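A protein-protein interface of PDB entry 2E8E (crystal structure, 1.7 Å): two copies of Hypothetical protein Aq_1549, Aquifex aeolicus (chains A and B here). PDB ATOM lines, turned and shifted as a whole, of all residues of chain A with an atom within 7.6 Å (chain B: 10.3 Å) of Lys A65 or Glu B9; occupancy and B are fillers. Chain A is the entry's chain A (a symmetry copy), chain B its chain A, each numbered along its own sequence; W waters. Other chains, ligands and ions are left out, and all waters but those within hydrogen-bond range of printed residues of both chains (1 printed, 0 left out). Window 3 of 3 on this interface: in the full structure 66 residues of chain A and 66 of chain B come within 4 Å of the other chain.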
ATOM      1  N   VAL A  61      -1.425   4.185 -37.237  1.00  0.00           N
ATOM      2  CA  VAL A  61      -2.447   4.427 -36.233  1.00  0.00           C
ATOM      3  C   VAL A  61      -3.754   4.978 -36.782  1.00  0.00           C
ATOM      4  O   VAL A  61      -3.778   6.019 -37.437  1.00  0.00           O
ATOM      5  CB  VAL A  61      -1.932   5.403 -35.156  1.00  0.00           C
ATOM      6  CG1 VAL A  61      -3.028   5.677 -34.134  1.00  0.00           C
ATOM      7  CG2 VAL A  61      -0.701   4.824 -34.481  1.00  0.00           C
ATOM      8  N   LYS A  62      -4.841   4.266 -36.506  1.00  0.00           N
ATOM      9  CA  LYS A  62      -6.164   4.697 -36.928  1.00  0.00           C
ATOM     10  C   LYS A  62      -6.766   5.474 -35.762  1.00  0.00           C
ATOM     11  O   LYS A  62      -7.481   6.457 -35.953  1.00  0.00           O
ATOM     12  CB  LYS A  62      -7.054   3.495 -37.249  1.00  0.00           C
ATOM     13  CG  LYS A  62      -8.489   3.877 -37.571  1.00  0.00           C
ATOM     14  CD  LYS A  62      -9.406   2.666 -37.647  1.00  0.00           C
ATOM     15  CE  LYS A  62      -8.995   1.710 -38.752  1.00  0.00           C
ATOM     16  NZ  LYS A  62      -9.969   0.587 -38.869  1.00  0.00           N
ATOM     17  N   ASP A  63      -6.461   5.028 -34.548  1.00  0.00           N
ATOM     18  CA  ASP A  63      -6.980   5.686 -33.357  1.00  0.00           C
ATOM     19  C   ASP A  63      -6.196   5.279 -32.115  1.00  0.00           C
ATOM     20  O   ASP A  63      -5.552   4.229 -32.077  1.00  0.00           O
ATOM     21  CB  ASP A  63      -8.462   5.336 -33.181  1.00  0.00           C
ATOM     22  CG  ASP A  63      -9.174   6.243 -32.183  1.00  0.00           C
ATOM     23  OD1 ASP A  63      -8.606   7.286 -31.799  1.00  0.00           O
ATOM     24  OD2 ASP A  63     -10.313   5.911 -31.795  1.00  0.00           O
ATOM     25  N   ILE A  64      -6.235   6.139 -31.105  1.00  0.00           N
ATOM     26  CA  ILE A  64      -5.568   5.875 -29.839  1.00  0.00           C
ATOM     27  C   ILE A  64      -6.593   6.264 -28.791  1.00  0.00           C
ATOM     28  O   ILE A  64      -7.079   7.394 -28.784  1.00  0.00           O
ATOM     29  CB  ILE A  64      -4.300   6.743 -29.648  1.00  0.00           C
ATOM     30  CG1 ILE A  64      -3.239   6.357 -30.678  1.00  0.00           C
ATOM     31  CG2 ILE A  64      -3.755   6.568 -28.226  1.00  0.00           C
ATOM     32  CD1 ILE A  64      -1.994   7.220 -30.644  1.00  0.00           C
ATOM     33  N   LYS A  65      -6.949   5.313 -27.935  1.00  0.00           N
ATOM     34  CA  LYS A  65      -7.916   5.564 -26.880  1.00  0.00           C
ATOM     35  C   LYS A  65      -7.216   5.380 -25.545  1.00  0.00           C
ATOM     36  O   LYS A  65      -6.475   4.417 -25.351  1.00  0.00           O
ATOM     37  CB  LYS A  65      -9.091   4.591 -26.985  1.00  0.00           C
ATOM     38  CG  LYS A  65      -9.891   4.714 -28.279  1.00  0.00           C
ATOM     39  CD  LYS A  65     -11.061   3.746 -28.285  1.00  0.00           C
ATOM     40  CE  LYS A  65     -11.898   3.893 -29.547  1.00  0.00           C
ATOM     41  NZ  LYS A  65     -13.012   2.900 -29.584  1.00  0.00           N
ATOM     42  N   ILE A  66      -7.438   6.312 -24.626  1.00  0.00           N
ATOM     43  CA  ILE A  66      -6.813   6.220 -23.316  1.00  0.00           C
ATOM     44  C   ILE A  66      -7.882   6.334 -22.244  1.00  0.00           C
ATOM     45  O   ILE A  66      -8.657   7.291 -22.219  1.00  0.00           O
ATOM     46  CB  ILE A  66      -5.761   7.328 -23.119  1.00  0.00           C
ATOM     47  CG1 ILE A  66      -4.779   7.329 -24.295  1.00  0.00           C
ATOM     48  CG2 ILE A  66      -4.997   7.086 -21.821  1.00  0.00           C
ATOM     49  CD1 ILE A  66      -3.757   8.455 -24.251  1.00  0.00           C
ATOM     50  N   PHE A  67      -7.922   5.343 -21.363  1.00  0.00           N
ATOM     51  CA  PHE A  67      -8.903   5.307 -20.297  1.00  0.00           C
ATOM     52  C   PHE A  67      -8.220   5.485 -18.955  1.00  0.00           C
ATOM     53  O   PHE A  67      -7.332   4.719 -18.597  1.00  0.00           O
ATOM     54  CB  PHE A  67      -9.647   3.971 -20.335  1.00  0.00           C
ATOM     55  CG  PHE A  67     -10.304   3.696 -21.656  1.00  0.00           C
ATOM     56  CD1 PHE A  67     -11.569   4.203 -21.939  1.00  0.00           C
ATOM     57  CD2 PHE A  67      -9.634   2.980 -22.642  1.00  0.00           C
ATOM     58  CE1 PHE A  67     -12.156   4.003 -23.191  1.00  0.00           C
ATOM     59  CE2 PHE A  67     -10.211   2.775 -23.893  1.00  0.00           C
ATOM     60  CZ  PHE A  67     -11.472   3.288 -24.168  1.00  0.00           C
ATOM     61  N   LEU A  68      -8.630   6.506 -18.213  1.00  0.00           N
ATOM     62  CA  LEU A  68      -8.043   6.746 -16.906  1.00  0.00           C
ATOM     63  C   LEU A  68      -9.089   6.643 -15.813  1.00  0.00           C
ATOM     64  O   LEU A  68     -10.190   7.171 -15.937  1.00  0.00           O
ATOM     65  CB  LEU A  68      -7.383   8.125 -16.850  1.00  0.00           C
ATOM     66  CG  LEU A  68      -6.224   8.346 -17.825  1.00  0.00           C
ATOM     67  CD1 LEU A  68      -6.738   9.029 -19.092  1.00  0.00           C
ATOM     68  CD2 LEU A  68      -5.159   9.196 -17.158  1.00  0.00           C
ATOM     69  N   ILE A  85      -4.360   3.543 -15.864  1.00  0.00           N
ATOM     70  CA  ILE A  85      -4.337   4.097 -17.205  1.00  0.00           C
ATOM     71  C   ILE A  85      -4.235   2.946 -18.185  1.00  0.00           C
ATOM     72  O   ILE A  85      -3.328   2.117 -18.085  1.00  0.00           O
ATOM     73  CB  ILE A  85      -3.127   5.028 -17.435  1.00  0.00           C
ATOM     74  CG1 ILE A  85      -3.071   6.110 -16.353  1.00  0.00           C
ATOM     75  CG2 ILE A  85      -3.235   5.671 -18.812  1.00  0.00           C
ATOM     76  CD1 ILE A  85      -1.886   7.047 -16.476  1.00  0.00           C
ATOM     77  N   LYS A  86      -5.172   2.897 -19.125  1.00  0.00           N
ATOM     78  CA  LYS A  86      -5.181   1.853 -20.138  1.00  0.00           C
ATOM     79  C   LYS A  86      -5.074   2.495 -21.515  1.00  0.00           C
ATOM     80  O   LYS A  86      -5.894   3.342 -21.876  1.00  0.00           O
ATOM     81  CB  LYS A  86      -6.473   1.037 -20.052  1.00  0.00           C
ATOM     82  CG  LYS A  86      -6.571  -0.078 -21.080  1.00  0.00           C
ATOM     83  CD  LYS A  86      -7.889  -0.827 -20.947  1.00  0.00           C
ATOM     84  CE  LYS A  86      -8.000  -1.928 -21.982  1.00  0.00           C
ATOM     85  NZ  LYS A  86      -6.877  -2.897 -21.862  1.00  0.00           N
ATOM     86  N   TYR A  87      -4.055   2.097 -22.270  1.00  0.00           N
ATOM     87  CA  TYR A  87      -3.833   2.623 -23.611  1.00  0.00           C
ATOM     88  C   TYR A  87      -4.287   1.588 -24.635  1.00  0.00           C
ATOM     89  O   TYR A  87      -3.893   0.424 -24.559  1.00  0.00           O
ATOM     90  CB  TYR A  87      -2.346   2.890 -23.846  1.00  0.00           C
ATOM     91  CG  TYR A  87      -1.709   3.876 -22.897  1.00  0.00           C
ATOM     92  CD1 TYR A  87      -1.559   5.216 -23.251  1.00  0.00           C
ATOM     93  CD2 TYR A  87      -1.232   3.464 -21.655  1.00  0.00           C
ATOM     94  CE1 TYR A  87      -0.939   6.124 -22.391  1.00  0.00           C
ATOM     95  CE2 TYR A  87      -0.617   4.362 -20.789  1.00  0.00           C
ATOM     96  CZ  TYR A  87      -0.470   5.687 -21.163  1.00  0.00           C
ATOM     97  OH  TYR A  87       0.161   6.568 -20.316  1.00  0.00           O
ATOM     98  N   VAL A  88      -5.104   2.016 -25.589  1.00  0.00           N
ATOM     99  CA  VAL A  88      -5.571   1.123 -26.641  1.00  0.00           C
ATOM    100  C   VAL A  88      -5.194   1.737 -27.984  1.00  0.00           C
ATOM    101  O   VAL A  88      -5.683   2.809 -28.345  1.00  0.00           O
ATOM    102  CB  VAL A  88      -7.108   0.925 -26.588  1.00  0.00           C
ATOM    103  CG1 VAL A  88      -7.561   0.051 -27.756  1.00  0.00           C
ATOM    104  CG2 VAL A  88      -7.511   0.284 -25.265  1.00  0.00           C
ATOM    105  N   ALA A  89      -4.302   1.073 -28.714  1.00  0.00           N
ATOM    106  CA  ALA A  89      -3.896   1.570 -30.022  1.00  0.00           C
ATOM    107  C   ALA A  89      -4.683   0.777 -31.055  1.00  0.00           C
ATOM    108  O   ALA A  89      -4.757  -0.448 -30.974  1.00  0.00           O
ATOM    109  CB  ALA A  89      -2.400   1.374 -30.230  1.00  0.00           C
ATOM    110  N   VAL A  90      -5.274   1.482 -32.012  1.00  0.00           N
ATOM    111  CA  VAL A  90      -6.080   0.848 -33.049  1.00  0.00           C
ATOM    112  C   VAL A  90      -5.446   1.064 -34.414  1.00  0.00           C
ATOM    113  O   VAL A  90      -5.142   2.196 -34.785  1.00  0.00           O
ATOM    114  CB  VAL A  90      -7.513   1.444 -33.070  1.00  0.00           C
ATOM    115  CG1 VAL A  90      -8.363   0.744 -34.118  1.00  0.00           C
ATOM    116  CG2 VAL A  90      -8.146   1.329 -31.687  1.00  0.00           C
ATOM    117  N   LEU A  98       3.703  -0.407 -29.142  1.00  0.00           N
ATOM    118  CA  LEU A  98       2.849   0.291 -28.183  1.00  0.00           C
ATOM    119  C   LEU A  98       3.478   0.215 -26.798  1.00  0.00           C
ATOM    120  O   LEU A  98       3.499   1.202 -26.065  1.00  0.00           O
ATOM    121  CB  LEU A  98       1.442  -0.315 -28.150  1.00  0.00           C
ATOM    122  CG  LEU A  98       0.502   0.349 -27.131  1.00  0.00           C
ATOM    123  CD1 LEU A  98       0.367   1.837 -27.447  1.00  0.00           C
ATOM    124  CD2 LEU A  98      -0.862  -0.324 -27.156  1.00  0.00           C
ATOM    125  N   SER A 125      -1.592  -0.287 -18.263  1.00  0.00           N
ATOM    126  CA  SER A 125      -1.856  -1.432 -19.127  1.00  0.00           C
ATOM    127  C   SER A 125      -2.072  -0.935 -20.546  1.00  0.00           C
ATOM    128  O   SER A 125      -2.339   0.244 -20.767  1.00  0.00           O
ATOM    129  CB  SER A 125      -3.094  -2.195 -18.658  1.00  0.00           C
ATOM    130  OG  SER A 125      -4.257  -1.396 -18.762  1.00  0.00           O
ATOM    131  N   GLU A 127      -3.068  -2.354 -24.923  1.00  0.00           N
ATOM    132  CA  GLU A 127      -3.476  -3.414 -25.823  1.00  0.00           C
ATOM    133  C   GLU A 127      -3.639  -2.855 -27.221  1.00  0.00           C
ATOM    134  O   GLU A 127      -3.904  -1.665 -27.406  1.00  0.00           O
ATOM    135  CB  GLU A 127      -4.793  -4.042 -25.362  1.00  0.00           C
ATOM    136  CG  GLU A 127      -6.007  -3.144 -25.495  1.00  0.00           C
ATOM    137  CD  GLU A 127      -7.294  -3.849 -25.101  1.00  0.00           C
ATOM    138  OE1 GLU A 127      -7.426  -4.231 -23.918  1.00  0.00           O
ATOM    139  OE2 GLU A 127      -8.172  -4.025 -25.972  1.00  0.00           O
ATOM    140  N   GLU A 131      -6.373  -3.346 -36.862  1.00  0.00           N
ATOM    141  CA  GLU A 131      -7.411  -2.971 -37.806  1.00  0.00           C
ATOM    142  C   GLU A 131      -6.870  -2.323 -39.066  1.00  0.00           C
ATOM    143  O   GLU A 131      -5.841  -1.646 -39.041  1.00  0.00           O
ATOM    144  CB  GLU A 131      -8.397  -2.001 -37.147  1.00  0.00           C
ATOM    145  CG  GLU A 131      -9.242  -2.618 -36.059  1.00  0.00           C
ATOM    146  CD  GLU A 131     -10.452  -1.772 -35.727  1.00  0.00           C
ATOM    147  OE1 GLU A 131     -10.940  -1.061 -36.632  1.00  0.00           O
ATOM    148  OE2 GLU A 131     -10.923  -1.836 -34.571  1.00  0.00           O
ATOM    149  N   VAL B   6     -12.177   9.283 -16.923  1.00  0.00           N
ATOM    150  CA  VAL B   6     -12.186  10.110 -18.117  1.00  0.00           C
ATOM    151  C   VAL B   6     -11.725   9.214 -19.252  1.00  0.00           C
ATOM    152  O   VAL B   6     -11.036   8.222 -19.023  1.00  0.00           O
ATOM    153  CB  VAL B   6     -11.257  11.345 -18.000  1.00  0.00           C
ATOM    154  CG1 VAL B   6     -11.746  12.259 -16.871  1.00  0.00           C
ATOM    155  CG2 VAL B   6      -9.825  10.912 -17.773  1.00  0.00           C
ATOM    156  N   GLU B   7     -12.137   9.544 -20.470  1.00  0.00           N
ATOM    157  CA  GLU B   7     -11.766   8.754 -21.634  1.00  0.00           C
ATOM    158  C   GLU B   7     -11.313   9.682 -22.747  1.00  0.00           C
ATOM    159  O   GLU B   7     -11.969  10.682 -23.044  1.00  0.00           O
ATOM    160  CB  GLU B   7     -12.955   7.913 -22.118  1.00  0.00           C
ATOM    161  CG  GLU B   7     -13.606   7.065 -21.034  1.00  0.00           C
ATOM    162  CD  GLU B   7     -14.639   6.098 -21.585  1.00  0.00           C
ATOM    163  OE1 GLU B   7     -15.454   6.518 -22.432  1.00  0.00           O
ATOM    164  OE2 GLU B   7     -14.640   4.921 -21.165  1.00  0.00           O
ATOM    165  N   LEU B   8     -10.186   9.342 -23.360  1.00  0.00           N
ATOM    166  CA  LEU B   8      -9.633  10.138 -24.444  1.00  0.00           C
ATOM    167  C   LEU B   8      -9.596   9.362 -25.747  1.00  0.00           C
ATOM    168  O   LEU B   8      -9.405   8.147 -25.757  1.00  0.00           O
ATOM    169  CB  LEU B   8      -8.211  10.592 -24.110  1.00  0.00           C
ATOM    170  CG  LEU B   8      -8.037  11.776 -23.157  1.00  0.00           C
ATOM    171  CD1 LEU B   8      -8.666  11.466 -21.806  1.00  0.00           C
ATOM    172  CD2 LEU B   8      -6.559  12.081 -23.007  1.00  0.00           C
ATOM    173  N   GLU B   9      -9.777  10.087 -26.845  1.00  0.00           N
ATOM    174  CA  GLU B   9      -9.742   9.500 -28.175  1.00  0.00           C
ATOM    175  C   GLU B   9      -9.072  10.504 -29.105  1.00  0.00           C
ATOM    176  O   GLU B   9      -9.298  11.710 -29.007  1.00  0.00           O
ATOM    177  CB  GLU B   9     -11.161   9.178 -28.653  1.00  0.00           C
ATOM    178  CG  GLU B   9     -11.227   8.572 -30.042  1.00  0.00           C
ATOM    179  CD  GLU B   9     -12.591   7.978 -30.346  1.00  0.00           C
ATOM    180  OE1 GLU B   9     -13.612   8.627 -30.025  1.00  0.00           O
ATOM    181  OE2 GLU B   9     -12.642   6.863 -30.912  1.00  0.00           O
ATOM    182  N   LEU B  10      -8.227  10.004 -30.000  1.00  0.00           N
ATOM    183  CA  LEU B  10      -7.518  10.861 -30.933  1.00  0.00           C
ATOM    184  C   LEU B  10      -8.531  11.697 -31.723  1.00  0.00           C
ATOM    185  O   LEU B  10      -9.540  11.174 -32.200  1.00  0.00           O
ATOM    186  CB  LEU B  10      -6.673   9.992 -31.867  1.00  0.00           C
ATOM    187  CG  LEU B  10      -5.470  10.592 -32.589  1.00  0.00           C
ATOM    188  CD1 LEU B  10      -4.463  11.138 -31.580  1.00  0.00           C
ATOM    189  CD2 LEU B  10      -4.832   9.505 -33.453  1.00  0.00           C
ATOM    190  N   SER B  11      -8.260  12.996 -31.839  1.00  0.00           N
ATOM    191  CA  SER B  11      -9.134  13.924 -32.556  1.00  0.00           C
ATOM    192  C   SER B  11      -8.432  14.496 -33.786  1.00  0.00           C
ATOM    193  O   SER B  11      -9.034  14.633 -34.851  1.00  0.00           O
ATOM    194  CB  SER B  11      -9.563  15.063 -31.628  1.00  0.00           C
ATOM    195  OG  SER B  11      -8.438  15.741 -31.095  1.00  0.00           O
ATOM    196  N   SER B  12      -7.162  14.847 -33.620  1.00  0.00           N
ATOM    197  CA  SER B  12      -6.336  15.371 -34.702  1.00  0.00           C
ATOM    198  C   SER B  12      -4.911  14.934 -34.382  1.00  0.00           C
ATOM    199  O   SER B  12      -4.701  14.180 -33.431  1.00  0.00           O
ATOM    200  CB  SER B  12      -6.433  16.901 -34.781  1.00  0.00           C
ATOM    201  OG  SER B  12      -5.929  17.528 -33.615  1.00  0.00           O
ATOM    202  N   GLU B  13      -3.936  15.389 -35.165  1.00  0.00           N
ATOM    203  CA  GLU B  13      -2.546  15.004 -34.932  1.00  0.00           C
ATOM    204  C   GLU B  13      -2.126  15.239 -33.485  1.00  0.00           C
ATOM    205  O   GLU B  13      -2.114  16.376 -33.011  1.00  0.00           O
ATOM    206  CB  GLU B  13      -1.608  15.778 -35.868  1.00  0.00           C
ATOM    207  CG  GLU B  13      -0.123  15.524 -35.621  1.00  0.00           C
ATOM    208  CD  GLU B  13       0.771  16.212 -36.639  1.00  0.00           C
ATOM    209  OE1 GLU B  13       0.643  17.443 -36.811  1.00  0.00           O
ATOM    210  OE2 GLU B  13       1.604  15.522 -37.266  1.00  0.00           O
ATOM    211  N   ALA B  14      -1.787  14.153 -32.796  1.00  0.00           N
ATOM    212  CA  ALA B  14      -1.347  14.201 -31.404  1.00  0.00           C
ATOM    213  C   ALA B  14      -2.273  15.033 -30.525  1.00  0.00           C
ATOM    214  O   ALA B  14      -1.816  15.746 -29.635  1.00  0.00           O
ATOM    215  CB  ALA B  14       0.074  14.753 -31.326  1.00  0.00           C
ATOM    216  N   THR B  15      -3.572  14.930 -30.778  1.00  0.00           N
ATOM    217  CA  THR B  15      -4.570  15.669 -30.015  1.00  0.00           C
ATOM    218  C   THR B  15      -5.707  14.726 -29.657  1.00  0.00           C
ATOM    219  O   THR B  15      -6.046  13.829 -30.429  1.00  0.00           O
ATOM    220  CB  THR B  15      -5.088  16.862 -30.825  1.00  0.00           C
ATOM    221  OG1 THR B  15      -3.966  17.625 -31.287  1.00  0.00           O
ATOM    222  CG2 THR B  15      -5.974  17.756 -29.964  1.00  0.00           C
ATOM    223  N   PHE B  16      -6.304  14.930 -28.487  1.00  0.00           N
ATOM    224  CA  PHE B  16      -7.360  14.042 -28.018  1.00  0.00           C
ATOM    225  C   PHE B  16      -8.643  14.709 -27.573  1.00  0.00           C
ATOM    226  O   PHE B  16      -8.607  15.728 -26.885  1.00  0.00           O
ATOM    227  CB  PHE B  16      -6.843  13.226 -26.830  1.00  0.00           C
ATOM    228  CG  PHE B  16      -5.648  12.388 -27.150  1.00  0.00           C
ATOM    229  CD1 PHE B  16      -5.799  11.049 -27.491  1.00  0.00           C
ATOM    230  CD2 PHE B  16      -4.378  12.948 -27.162  1.00  0.00           C
ATOM    231  CE1 PHE B  16      -4.694  10.276 -27.844  1.00  0.00           C
ATOM    232  CE2 PHE B  16      -3.264  12.185 -27.516  1.00  0.00           C
ATOM    233  CZ  PHE B  16      -3.429  10.844 -27.858  1.00  0.00           C
ATOM    234  N   LEU B  17      -9.772  14.131 -27.972  1.00  0.00           N
ATOM    235  CA  LEU B  17     -11.062  14.623 -27.519  1.00  0.00           C
ATOM    236  C   LEU B  17     -11.179  13.902 -26.182  1.00  0.00           C
ATOM    237  O   LEU B  17     -11.139  12.667 -26.114  1.00  0.00           O
ATOM    238  CB  LEU B  17     -12.180  14.225 -28.486  1.00  0.00           C
ATOM    239  CG  LEU B  17     -12.478  15.351 -29.484  1.00  0.00           C
ATOM    240  CD1 LEU B  17     -13.376  14.849 -30.613  1.00  0.00           C
ATOM    241  CD2 LEU B  17     -13.144  16.512 -28.744  1.00  0.00           C
ATOM    242  N   SER B  18     -11.291  14.690 -25.119  1.00  0.00           N
ATOM    243  CA  SER B  18     -11.329  14.165 -23.766  1.00  0.00           C
ATOM    244  C   SER B  18     -12.692  14.286 -23.107  1.00  0.00           C
ATOM    245  O   SER B  18     -13.165  15.391 -22.833  1.00  0.00           O
ATOM    246  CB  SER B  18     -10.276  14.901 -22.941  1.00  0.00           C
ATOM    247  OG  SER B  18      -9.055  14.962 -23.662  1.00  0.00           O
ATOM    248  N   LYS B  19     -13.297  13.132 -22.845  1.00  0.00           N
ATOM    249  CA  LYS B  19     -14.619  13.040 -22.238  1.00  0.00           C
ATOM    250  C   LYS B  19     -14.611  13.081 -20.713  1.00  0.00           C
ATOM    251  O   LYS B  19     -13.973  12.256 -20.060  1.00  0.00           O
ATOM    252  CB  LYS B  19     -15.313  11.756 -22.701  1.00  0.00           C
ATOM    253  CG  LYS B  19     -16.713  11.567 -22.133  1.00  0.00           C
ATOM    254  CD  LYS B  19     -17.383  10.321 -22.701  1.00  0.00           C
ATOM    255  CE  LYS B  19     -18.824  10.205 -22.229  1.00  0.00           C
ATOM    256  NZ  LYS B  19     -19.505   8.991 -22.771  1.00  0.00           N
ATOM    257  N   THR B  20     -15.333  14.049 -20.160  1.00  0.00           N
ATOM    258  CA  THR B  20     -15.451  14.217 -18.715  1.00  0.00           C
ATOM    259  C   THR B  20     -16.940  14.285 -18.380  1.00  0.00           C
ATOM    260  O   THR B  20     -17.785  14.184 -19.273  1.00  0.00           O
ATOM    261  CB  THR B  20     -14.785  15.522 -18.244  1.00  0.00           C
ATOM    262  OG1 THR B  20     -15.601  16.638 -18.617  1.00  0.00           O
ATOM    263  CG2 THR B  20     -13.406  15.678 -18.889  1.00  0.00           C
ATOM    264  N   GLU B  24     -16.882  17.328 -23.405  1.00  0.00           N
ATOM    265  CA  GLU B  24     -15.617  16.966 -24.026  1.00  0.00           C
ATOM    266  C   GLU B  24     -14.796  18.174 -24.459  1.00  0.00           C
ATOM    267  O   GLU B  24     -15.327  19.146 -24.998  1.00  0.00           O
ATOM    268  CB  GLU B  24     -15.886  16.072 -25.240  1.00  0.00           C
ATOM    269  CG  GLU B  24     -16.688  14.822 -24.917  1.00  0.00           C
ATOM    270  CD  GLU B  24     -17.157  14.082 -26.160  1.00  0.00           C
ATOM    271  OE1 GLU B  24     -17.899  14.678 -26.965  1.00  0.00           O
ATOM    272  OE2 GLU B  24     -16.791  12.902 -26.328  1.00  0.00           O
ATOM    273  N   ILE B  25     -13.492  18.108 -24.213  1.00  0.00           N
ATOM    274  CA  ILE B  25     -12.592  19.175 -24.611  1.00  0.00           C
ATOM    275  C   ILE B  25     -11.446  18.543 -25.376  1.00  0.00           C
ATOM    276  O   ILE B  25     -11.177  17.355 -25.217  1.00  0.00           O
ATOM    277  CB  ILE B  25     -12.014  19.936 -23.396  1.00  0.00           C
ATOM    278  CG1 ILE B  25     -11.400  18.952 -22.402  1.00  0.00           C
ATOM    279  CG2 ILE B  25     -13.107  20.761 -22.740  1.00  0.00           C
ATOM    280  CD1 ILE B  25     -10.701  19.630 -21.237  1.00  0.00           C
ATOM    281  N   THR B  26     -10.786  19.331 -26.215  1.00  0.00           N
ATOM    282  CA  THR B  26      -9.659  18.830 -26.981  1.00  0.00           C
ATOM    283  C   THR B  26      -8.385  19.208 -26.252  1.00  0.00           C
ATOM    284  O   THR B  26      -8.162  20.374 -25.932  1.00  0.00           O
ATOM    285  CB  THR B  26      -9.625  19.414 -28.412  1.00  0.00           C
ATOM    286  OG1 THR B  26      -9.636  20.845 -28.352  1.00  0.00           O
ATOM    287  CG2 THR B  26     -10.823  18.926 -29.207  1.00  0.00           C
ATOM    288  N   ALA B  27      -7.561  18.204 -25.976  1.00  0.00           N
ATOM    289  CA  ALA B  27      -6.309  18.417 -25.270  1.00  0.00           C
ATOM    290  C   ALA B  27      -5.164  17.778 -26.035  1.00  0.00           C
ATOM    291  O   ALA B  27      -5.246  16.617 -26.435  1.00  0.00           O
ATOM    292  CB  ALA B  27      -6.395  17.815 -23.875  1.00  0.00           C
ATOM    293  N   GLY B  28      -4.093  18.536 -26.230  1.00  0.00           N
ATOM    294  CA  GLY B  28      -2.956  17.996 -26.945  1.00  0.00           C
ATOM    295  C   GLY B  28      -2.250  19.021 -27.802  1.00  0.00           C
ATOM    296  O   GLY B  28      -2.393  20.225 -27.608  1.00  0.00           O
HETATM  297  O   HOH W   1     -14.767   5.455 -31.153  1.00  0.00           O
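The backbone NH (N) of Val B6 sits at hydrogen-bond distance from the backbone carbonyl oxygen (O) of Leu A68, at 3.1 Å. The backbone carbonyl oxygen (O) of Ile A66 lies within hydrogen-bond range of the backbone NH (N) of Leu B8. The side-chain carboxylate of Glu B9 sits close to the side-chain carboxylate of Asp A63, at 2.7 Å. The backbone NH of Leu B10 lies within hydrogen-bond range of the side-chain carboxylate of Asp A63. The backbone carbonyl oxygen (O) of Ile A64 lies within hydrogen-bond range of the backbone NH (N) of Leu B10, 3.1 Å away.
O of Glu B9 is in hydrogen-bond range of N of Leu B17 (2.7 Å). The side-chain hydroxyl (OG) of Ser B11 lies within hydrogen-bond range of the backbone NH (N) of Phe B16 (3.5 Å). O of Phe B16 is in hydrogen-bond range of OG of Ser B18. The backbone carbonyl oxygen (O) of Asp A63 is in hydrogen-bond range of the backbone NH (N) of Val A90, 2.8 Å away. The backbone carbonyl oxygen of Lys A65 is in hydrogen-bond range of the backbone NH of Val A88 (2.8 Å). The backbone carbonyl oxygen (O) of Phe A67 sits at hydrogen-bond distance from the backbone NH (N) of Lys A86.
Among the printed residues, merely in contact across the chains: Lys A65 with Leu B8, Phe A67 with Glu B7, Lys A65 with Glu B9, Ile A64 with Glu B9, Ile A66 with Glu B7, Phe A67 with Val B6, Ile A64 with Phe B16 and Ile A64 with Leu B8.
Printed residues of chain B within 4 Å of Asp A63: Glu B9 (2.7 Å) and Leu B10 (3.3 Å). Ile A64 touches just these residues of chain B: Leu B8 (3.9 Å), Glu B9 (3.4 Å), Leu B10 (3.1 Å) and Phe B16 (3.8 Å). Of chain B, only Leu B8 (3.2 Å) and Glu B9 (3.4 Å) come within 4 Å of Lys A65. Of the printed residues of chain B, Phe A67 touches Val B6 (3.8 Å) and Glu B7 (3.2 Å). Of the printed residues of chain B, Leu A68 touches Val B6 (3.1 Å). Printed residues of chain A within 4 Å of Leu B8: Ile A64, Lys A65 and Ile A66. Printed residues of chain A within 4 Å of Glu B9: Asp A63 (2.7 Å), Ile A64 (3.4 Å) and Lys A65 (3.4 Å). Printed residues of chain A within 4 Å of Phe B16: Ile A64. Glu B24 touches none of the printed residues of chain A. The nearest residue of chain B that does not touch Lys A65 is Leu B10 (5.3 Å). The nearest printed residue of chain B that does not touch Asp A63 is Ser B11 (5.7 Å).
Printed residues of chain A that touch a printed residue of chain B: Asp A63, Ile A64, Lys A65, Ile A66, Phe A67 and Leu A68. Hydrophobic or aromatic side chains of chain A that line the printed part of chain B: Ile A64, Phe A67 and Leu A68.
No position is printed for both chains. Of the 13 pairs that touch across the chains among the printed residues, none has its exchanged pair printed and touching as well.
Water W1 bridges the side-chain carboxylate (OE2) of Glu B9 (2.6 Å) and the side-chain amino group (NZ) of Lys A65 (3.5 Å).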
